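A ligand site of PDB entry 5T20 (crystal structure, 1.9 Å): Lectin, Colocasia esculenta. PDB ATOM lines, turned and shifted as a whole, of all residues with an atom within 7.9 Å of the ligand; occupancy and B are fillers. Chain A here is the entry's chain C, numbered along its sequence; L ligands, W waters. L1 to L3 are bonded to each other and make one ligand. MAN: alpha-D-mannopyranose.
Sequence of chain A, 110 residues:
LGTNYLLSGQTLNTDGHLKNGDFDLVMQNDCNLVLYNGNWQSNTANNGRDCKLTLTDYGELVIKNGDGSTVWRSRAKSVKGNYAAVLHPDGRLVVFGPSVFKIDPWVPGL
OD1 of Asn 39 touches O4 of MAN L3, at 3.7 Å. Ala 45 touches the ligand. Of the 21 residues printed, 8 come within 4 Å of the ligand.
The side-chain amide nitrogen (NE2) of Gln 28 lies within hydrogen-bond range of the side-chain hydroxyl (OH) of Tyr 36 (2.6 Å). ND2 of Asn 32 lies within hydrogen-bond range of OE1 of Gln 41, at 2.8 Å. The side-chain amide oxygen (OD1) of Asn 43 sits close to the side-chain amide oxygen (OE1) of Gln 41 (2.9 Å). The side-chain carboxylate (OD1) of Asp 30 sits close to the side-chain amide oxygen (OE1) of Gln 28. N of Asn 32 sits at hydrogen-bond distance from OD1 of Asp 30 (3.1 Å). The side-chain carboxylate of Asp 15 lies within hydrogen-bond range of the backbone NH of Asn 29 (3.3 Å). The backbone NH (N) of Thr 44 lies within hydrogen-bond range of the side-chain amide oxygen (OD1) of Asn 32 (3.1 Å). The side-chain amide oxygen of Asn 32 lies within hydrogen-bond range of the backbone NH of Asn 43 (3.0 Å).
An oxygen (O4) of MAN L2 lies within hydrogen-bond range of the side-chain hydroxyl (OH) of Tyr 36 (2.5 Å). NE2 of Gln 41 sits at hydrogen-bond distance from O6 of MAN L2 (2.6 Å). OD2 of Asp 30 lies within hydrogen-bond range of O2 of MAN L2 (2.7 Å). The side-chain amide oxygen of Asn 29 sits at hydrogen-bond distance from an oxygen (O3) of MAN L1, 2.8 Å away. An oxygen (O3) of MAN L2 lies close to the side-chain amide oxygen of Gln 28 (3.0 Å). ND2 of Asn 32 is in hydrogen-bond range of O2 of MAN L2 (3.0 Å).
Water W2 lies within hydrogen-bond range of the side-chain carboxylate (OD2) of Asp 30 (2.6 Å) and the side-chain amide oxygen (OD1) of Asn 46 (2.7 Å).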
ATOM      1  N   ASP A  15      14.562  -5.632  26.271  1.00  0.00           N
ATOM      2  CA  ASP A  15      14.157  -5.708  27.698  1.00  0.00           C
ATOM      3  C   ASP A  15      12.658  -6.171  27.865  1.00  0.00           C
ATOM      4  O   ASP A  15      12.079  -6.075  28.956  1.00  0.00           O
ATOM      5  CB  ASP A  15      14.459  -4.397  28.475  1.00  0.00           C
ATOM      6  CG  ASP A  15      15.928  -4.008  28.469  1.00  0.00           C
ATOM      7  OD1 ASP A  15      16.772  -4.871  28.801  1.00  0.00           O
ATOM      8  OD2 ASP A  15      16.234  -2.849  28.170  1.00  0.00           O
ATOM      9  N   VAL A  26      13.140 -13.344  28.509  1.00  0.00           N
ATOM     10  CA  VAL A  26      13.540 -11.943  28.351  1.00  0.00           C
ATOM     11  C   VAL A  26      14.452 -11.760  27.142  1.00  0.00           C
ATOM     12  O   VAL A  26      15.482 -12.433  27.053  1.00  0.00           O
ATOM     13  CB  VAL A  26      14.217 -11.365  29.634  1.00  0.00           C
ATOM     14  CG1 VAL A  26      14.400  -9.854  29.533  1.00  0.00           C
ATOM     15  CG2 VAL A  26      13.424 -11.716  30.903  1.00  0.00           C
ATOM     16  N   MET A  27      14.110 -10.808  26.273  1.00  0.00           N
ATOM     17  CA  MET A  27      14.943 -10.374  25.144  1.00  0.00           C
ATOM     18  C   MET A  27      15.780  -9.242  25.730  1.00  0.00           C
ATOM     19  O   MET A  27      15.335  -8.117  25.796  1.00  0.00           O
ATOM     20  CB  MET A  27      14.074  -9.950  23.941  1.00  0.00           C
ATOM     21  CG  MET A  27      14.861  -9.339  22.808  1.00  0.00           C
ATOM     22  SD  MET A  27      15.754 -10.590  21.868  1.00  0.00           S
ATOM     23  CE  MET A  27      17.303 -10.594  22.671  1.00  0.00           C
ATOM     24  N   GLN A  28      16.941  -9.577  26.263  1.00  0.00           N
ATOM     25  CA  GLN A  28      17.745  -8.658  27.043  1.00  0.00           C
ATOM     26  C   GLN A  28      18.497  -7.595  26.261  1.00  0.00           C
ATOM     27  O   GLN A  28      18.723  -7.725  25.058  1.00  0.00           O
ATOM     28  CB  GLN A  28      18.730  -9.453  27.903  1.00  0.00           C
ATOM     29  CG  GLN A  28      18.029 -10.368  28.898  1.00  0.00           C
ATOM     30  CD  GLN A  28      18.980 -11.126  29.770  1.00  0.00           C
ATOM     31  OE1 GLN A  28      20.179 -11.339  29.459  1.00  0.00           O
ATOM     32  NE2 GLN A  28      18.480 -11.548  30.871  1.00  0.00           N
ATOM     33  N   ASN A  29      18.948  -6.551  27.000  1.00  0.00           N
ATOM     34  CA  ASN A  29      19.728  -5.422  26.497  1.00  0.00           C
ATOM     35  C   ASN A  29      21.095  -5.882  25.994  1.00  0.00           C
ATOM     36  O   ASN A  29      21.650  -5.243  25.093  1.00  0.00           O
ATOM     37  CB  ASN A  29      19.895  -4.354  27.593  1.00  0.00           C
ATOM     38  CG  ASN A  29      20.622  -4.858  28.831  1.00  0.00           C
ATOM     39  OD1 ASN A  29      20.387  -5.975  29.304  1.00  0.00           O
ATOM     40  ND2 ASN A  29      21.542  -4.072  29.375  1.00  0.00           N
ATOM     41  N   ASP A  30      21.634  -6.999  26.548  1.00  0.00           N
ATOM     42  CA  ASP A  30      22.918  -7.549  26.117  1.00  0.00           C
ATOM     43  C   ASP A  30      22.763  -8.520  24.917  1.00  0.00           C
ATOM     44  O   ASP A  30      23.732  -9.205  24.586  1.00  0.00           O
ATOM     45  CB  ASP A  30      23.641  -8.258  27.289  1.00  0.00           C
ATOM     46  CG  ASP A  30      23.115  -9.642  27.681  1.00  0.00           C
ATOM     47  OD1 ASP A  30      21.969  -9.974  27.313  1.00  0.00           O
ATOM     48  OD2 ASP A  30      23.855 -10.377  28.345  1.00  0.00           O
ATOM     49  N   CYS A  31      21.551  -8.617  24.304  1.00  0.00           N
ATOM     50  CA  CYS A  31      21.216  -9.440  23.106  1.00  0.00           C
ATOM     51  C   CYS A  31      20.948 -10.923  23.445  1.00  0.00           C
ATOM     52  O   CYS A  31      20.680 -11.717  22.544  1.00  0.00           O
ATOM     53  CB  CYS A  31      22.280  -9.327  22.025  1.00  0.00           C
ATOM     54  SG  CYS A  31      21.637  -9.486  20.332  1.00  0.00           S
ATOM     55  N   ASN A  32      21.069 -11.315  24.707  1.00  0.00           N
ATOM     56  CA  ASN A  32      20.800 -12.712  25.049  1.00  0.00           C
ATOM     57  C   ASN A  32      19.316 -12.901  25.299  1.00  0.00           C
ATOM     58  O   ASN A  32      18.707 -12.122  26.043  1.00  0.00           O
ATOM     59  CB  ASN A  32      21.615 -13.168  26.274  1.00  0.00           C
ATOM     60  CG  ASN A  32      21.908 -14.656  26.335  1.00  0.00           C
ATOM     61  OD1 ASN A  32      21.615 -15.424  25.406  1.00  0.00           O
ATOM     62  ND2 ASN A  32      22.486 -15.118  27.439  1.00  0.00           N
ATOM     63  N   LEU A  33      18.719 -13.904  24.639  1.00  0.00           N
ATOM     64  CA  LEU A  33      17.304 -14.221  24.846  1.00  0.00           C
ATOM     65  C   LEU A  33      17.280 -15.326  25.870  1.00  0.00           C
ATOM     66  O   LEU A  33      17.730 -16.421  25.569  1.00  0.00           O
ATOM     67  CB  LEU A  33      16.605 -14.610  23.514  1.00  0.00           C
ATOM     68  CG  LEU A  33      15.137 -15.109  23.593  1.00  0.00           C
ATOM     69  CD1 LEU A  33      14.151 -13.957  23.942  1.00  0.00           C
ATOM     70  CD2 LEU A  33      14.714 -15.713  22.248  1.00  0.00           C
ATOM     71  N   VAL A  34      16.855 -15.005  27.102  1.00  0.00           N
ATOM     72  CA  VAL A  34      16.964 -15.953  28.211  1.00  0.00           C
ATOM     73  C   VAL A  34      15.602 -16.333  28.764  1.00  0.00           C
ATOM     74  O   VAL A  34      14.805 -15.468  29.119  1.00  0.00           O
ATOM     75  CB  VAL A  34      17.873 -15.385  29.355  1.00  0.00           C
ATOM     76  CG1 VAL A  34      18.034 -16.401  30.495  1.00  0.00           C
ATOM     77  CG2 VAL A  34      19.231 -14.948  28.836  1.00  0.00           C
ATOM     78  N   LEU A  35      15.376 -17.653  28.872  1.00  0.00           N
ATOM     79  CA  LEU A  35      14.187 -18.254  29.461  1.00  0.00           C
ATOM     80  C   LEU A  35      14.520 -18.572  30.923  1.00  0.00           C
ATOM     81  O   LEU A  35      15.019 -19.656  31.232  1.00  0.00           O
ATOM     82  CB  LEU A  35      13.765 -19.503  28.641  1.00  0.00           C
ATOM     83  CG  LEU A  35      12.473 -20.303  29.022  1.00  0.00           C
ATOM     84  CD1 LEU A  35      11.393 -19.431  29.642  1.00  0.00           C
ATOM     85  CD2 LEU A  35      11.934 -21.060  27.822  1.00  0.00           C
ATOM     86  N   TYR A  36      14.308 -17.601  31.808  1.00  0.00           N
ATOM     87  CA  TYR A  36      14.604 -17.753  33.226  1.00  0.00           C
ATOM     88  C   TYR A  36      13.741 -18.820  33.837  1.00  0.00           C
ATOM     89  O   TYR A  36      12.539 -18.868  33.543  1.00  0.00           O
ATOM     90  CB  TYR A  36      14.491 -16.408  33.977  1.00  0.00           C
ATOM     91  CG  TYR A  36      15.694 -15.546  33.672  1.00  0.00           C
ATOM     92  CD1 TYR A  36      16.928 -15.782  34.287  1.00  0.00           C
ATOM     93  CD2 TYR A  36      15.632 -14.527  32.732  1.00  0.00           C
ATOM     94  CE1 TYR A  36      18.048 -15.010  33.986  1.00  0.00           C
ATOM     95  CE2 TYR A  36      16.739 -13.717  32.454  1.00  0.00           C
ATOM     96  CZ  TYR A  36      17.945 -13.955  33.094  1.00  0.00           C
ATOM     97  OH  TYR A  36      19.076 -13.206  32.840  1.00  0.00           O
ATOM     98  N   ASN A  37      14.394 -19.753  34.567  1.00  0.00           N
ATOM     99  CA  ASN A  37      13.860 -20.949  35.231  1.00  0.00           C
ATOM    100  C   ASN A  37      13.544 -22.068  34.233  1.00  0.00           C
ATOM    101  O   ASN A  37      13.103 -23.138  34.658  1.00  0.00           O
ATOM    102  CB  ASN A  37      12.643 -20.623  36.122  1.00  0.00           C
ATOM    103  CG  ASN A  37      12.989 -19.784  37.318  1.00  0.00           C
ATOM    104  OD1 ASN A  37      13.972 -20.029  38.021  1.00  0.00           O
ATOM    105  ND2 ASN A  37      12.173 -18.773  37.594  1.00  0.00           N
ATOM    106  N   GLY A  38      13.865 -21.861  32.959  1.00  0.00           N
ATOM    107  CA  GLY A  38      13.602 -22.830  31.903  1.00  0.00           C
ATOM    108  C   GLY A  38      14.838 -23.460  31.314  1.00  0.00           C
ATOM    109  O   GLY A  38      14.743 -24.169  30.309  1.00  0.00           O
ATOM    110  N   ASN A  39      16.018 -23.197  31.914  1.00  0.00           N
ATOM    111  CA  ASN A  39      17.335 -23.738  31.525  1.00  0.00           C
ATOM    112  C   ASN A  39      17.543 -23.618  29.999  1.00  0.00           C
ATOM    113  O   ASN A  39      17.875 -24.587  29.326  1.00  0.00           O
ATOM    114  CB  ASN A  39      17.451 -25.204  32.004  1.00  0.00           C
ATOM    115  CG  ASN A  39      18.834 -25.797  31.923  1.00  0.00           C
ATOM    116  OD1 ASN A  39      19.847 -25.146  32.196  1.00  0.00           O
ATOM    117  ND2 ASN A  39      18.895 -27.065  31.560  1.00  0.00           N
ATOM    118  N   TRP A  40      17.269 -22.423  29.452  1.00  0.00           N
ATOM    119  CA  TRP A  40      17.444 -22.200  28.038  1.00  0.00           C
ATOM    120  C   TRP A  40      17.765 -20.751  27.781  1.00  0.00           C
ATOM    121  O   TRP A  40      17.185 -19.851  28.418  1.00  0.00           O
ATOM    122  CB  TRP A  40      16.189 -22.631  27.234  1.00  0.00           C
ATOM    123  CG  TRP A  40      16.424 -22.607  25.758  1.00  0.00           C
ATOM    124  CD1 TRP A  40      16.902 -23.632  24.982  1.00  0.00           C
ATOM    125  CD2 TRP A  40      16.301 -21.462  24.880  1.00  0.00           C
ATOM    126  NE1 TRP A  40      17.027 -23.220  23.680  1.00  0.00           N
ATOM    127  CE2 TRP A  40      16.679 -21.884  23.587  1.00  0.00           C
ATOM    128  CE3 TRP A  40      15.862 -20.138  25.067  1.00  0.00           C
ATOM    129  CZ2 TRP A  40      16.639 -21.031  22.485  1.00  0.00           C
ATOM    130  CZ3 TRP A  40      15.873 -19.281  23.974  1.00  0.00           C
ATOM    131  CH2 TRP A  40      16.234 -19.738  22.695  1.00  0.00           C
ATOM    132  N   GLN A  41      18.690 -20.530  26.842  1.00  0.00           N
ATOM    133  CA  GLN A  41      19.093 -19.216  26.342  1.00  0.00           C
ATOM    134  C   GLN A  41      19.544 -19.358  24.901  1.00  0.00           C
ATOM    135  O   GLN A  41      19.969 -20.451  24.511  1.00  0.00           O
ATOM    136  CB  GLN A  41      20.192 -18.569  27.213  1.00  0.00           C
ATOM    137  CG  GLN A  41      21.433 -19.423  27.396  1.00  0.00           C
ATOM    138  CD  GLN A  41      22.544 -18.650  28.058  1.00  0.00           C
ATOM    139  OE1 GLN A  41      23.231 -17.832  27.436  1.00  0.00           O
ATOM    140  NE2 GLN A  41      22.750 -18.925  29.331  1.00  0.00           N
ATOM    141  N   ASN A  43      22.156 -17.915  23.839  1.00  0.00           N
ATOM    142  CA  ASN A  43      23.628 -17.870  23.977  1.00  0.00           C
ATOM    143  C   ASN A  43      24.240 -16.807  23.061  1.00  0.00           C
ATOM    144  O   ASN A  43      25.270 -17.048  22.423  1.00  0.00           O
ATOM    145  CB  ASN A  43      24.272 -19.251  23.714  1.00  0.00           C
ATOM    146  CG  ASN A  43      24.348 -20.106  24.944  1.00  0.00           C
ATOM    147  OD1 ASN A  43      24.909 -19.714  25.961  1.00  0.00           O
ATOM    148  ND2 ASN A  43      23.789 -21.304  24.865  1.00  0.00           N
ATOM    149  N   THR A  44      23.614 -15.624  23.035  1.00  0.00           N
ATOM    150  CA  THR A  44      24.014 -14.513  22.198  1.00  0.00           C
ATOM    151  C   THR A  44      24.288 -13.259  23.024  1.00  0.00           C
ATOM    152  O   THR A  44      24.132 -12.153  22.506  1.00  0.00           O
ATOM    153  CB  THR A  44      22.964 -14.290  21.096  1.00  0.00           C
ATOM    154  OG1 THR A  44      21.681 -14.244  21.736  1.00  0.00           O
ATOM    155  CG2 THR A  44      22.963 -15.392  20.035  1.00  0.00           C
ATOM    156  N   ALA A  45      24.780 -13.418  24.266  1.00  0.00           N
ATOM    157  CA  ALA A  45      25.152 -12.290  25.113  1.00  0.00           C
ATOM    158  C   ALA A  45      26.316 -11.520  24.474  1.00  0.00           C
ATOM    159  O   ALA A  45      27.273 -12.137  23.991  1.00  0.00           O
ATOM    160  CB  ALA A  45      25.531 -12.772  26.515  1.00  0.00           C
ATOM    161  N   ASN A  46      26.206 -10.168  24.424  1.00  0.00           N
ATOM    162  CA  ASN A  46      27.172  -9.228  23.844  1.00  0.00           C
ATOM    163  C   ASN A  46      27.274  -9.343  22.309  1.00  0.00           C
ATOM    164  O   ASN A  46      28.246  -8.837  21.721  1.00  0.00           O
ATOM    165  CB  ASN A  46      28.579  -9.424  24.459  1.00  0.00           C
ATOM    166  CG  ASN A  46      28.618  -9.633  25.949  1.00  0.00           C
ATOM    167  OD1 ASN A  46      27.826  -9.059  26.705  1.00  0.00           O
ATOM    168  ND2 ASN A  46      29.486 -10.555  26.395  1.00  0.00           N
HETATM  169  C1  MAN L   1      22.351 -10.756  32.722  1.00  0.00           C
HETATM  170  C2  MAN L   1      21.239  -9.704  32.632  1.00  0.00           C
HETATM  171  C3  MAN L   1      21.549  -8.705  31.494  1.00  0.00           C
HETATM  172  C4  MAN L   1      22.918  -8.072  31.723  1.00  0.00           C
HETATM  173  C5  MAN L   1      23.978  -9.191  31.793  1.00  0.00           C
HETATM  174  C6  MAN L   1      25.364  -8.590  31.975  1.00  0.00           C
HETATM  175  O2  MAN L   1      21.114  -8.998  33.880  1.00  0.00           O
HETATM  176  O3  MAN L   1      20.577  -7.646  31.505  1.00  0.00           O
HETATM  177  O4  MAN L   1      23.201  -7.135  30.622  1.00  0.00           O
HETATM  178  O5  MAN L   1      23.675 -10.118  32.872  1.00  0.00           O
HETATM  179  O6  MAN L   1      25.432  -7.950  33.253  1.00  0.00           O
HETATM  180  C1  MAN L   2      24.666 -14.286  30.401  1.00  0.00           C
HETATM  181  C2  MAN L   2      23.942 -12.921  30.397  1.00  0.00           C
HETATM  182  C3  MAN L   2      23.085 -12.780  31.643  1.00  0.00           C
HETATM  183  C4  MAN L   2      22.161 -13.987  31.765  1.00  0.00           C
HETATM  184  C5  MAN L   2      22.939 -15.305  31.682  1.00  0.00           C
HETATM  185  C6  MAN L   2      21.951 -16.481  31.660  1.00  0.00           C
HETATM  186  O1  MAN L   2      25.575 -14.376  31.493  1.00  0.00           O
HETATM  187  O2  MAN L   2      23.105 -12.831  29.235  1.00  0.00           O
HETATM  188  O3  MAN L   2      22.278 -11.584  31.539  1.00  0.00           O
HETATM  189  O4  MAN L   2      21.518 -13.905  33.020  1.00  0.00           O
HETATM  190  O5  MAN L   2      23.730 -15.346  30.474  1.00  0.00           O
HETATM  191  O6  MAN L   2      22.676 -17.726  31.650  1.00  0.00           O
HETATM  192  C1  MAN L   3      23.084 -18.101  33.010  1.00  0.00           C
HETATM  193  C2  MAN L   3      24.185 -19.209  33.017  1.00  0.00           C
HETATM  194  C3  MAN L   3      23.589 -20.583  32.623  1.00  0.00           C
HETATM  195  C4  MAN L   3      22.301 -20.891  33.387  1.00  0.00           C
HETATM  196  C5  MAN L   3      21.372 -19.709  33.218  1.00  0.00           C
HETATM  197  C6  MAN L   3      20.009 -20.002  33.842  1.00  0.00           C
HETATM  198  O2  MAN L   3      24.780 -19.305  34.320  1.00  0.00           O
HETATM  199  O3  MAN L   3      24.548 -21.642  32.843  1.00  0.00           O
HETATM  200  O4  MAN L   3      21.697 -22.056  32.829  1.00  0.00           O
HETATM  201  O5  MAN L   3      21.973 -18.540  33.790  1.00  0.00           O
HETATM  202  O6  MAN L   3      20.099 -19.892  35.258  1.00  0.00           O
HETATM  203  O   HOH W   1      25.677 -11.766  34.600  1.00  0.00           O
HETATM  204  O   HOH W   2      26.283  -9.739  28.830  1.00  0.00           O
HETATM  205  O   HOH W   3      20.502  -6.366  34.289  1.00  0.00           O
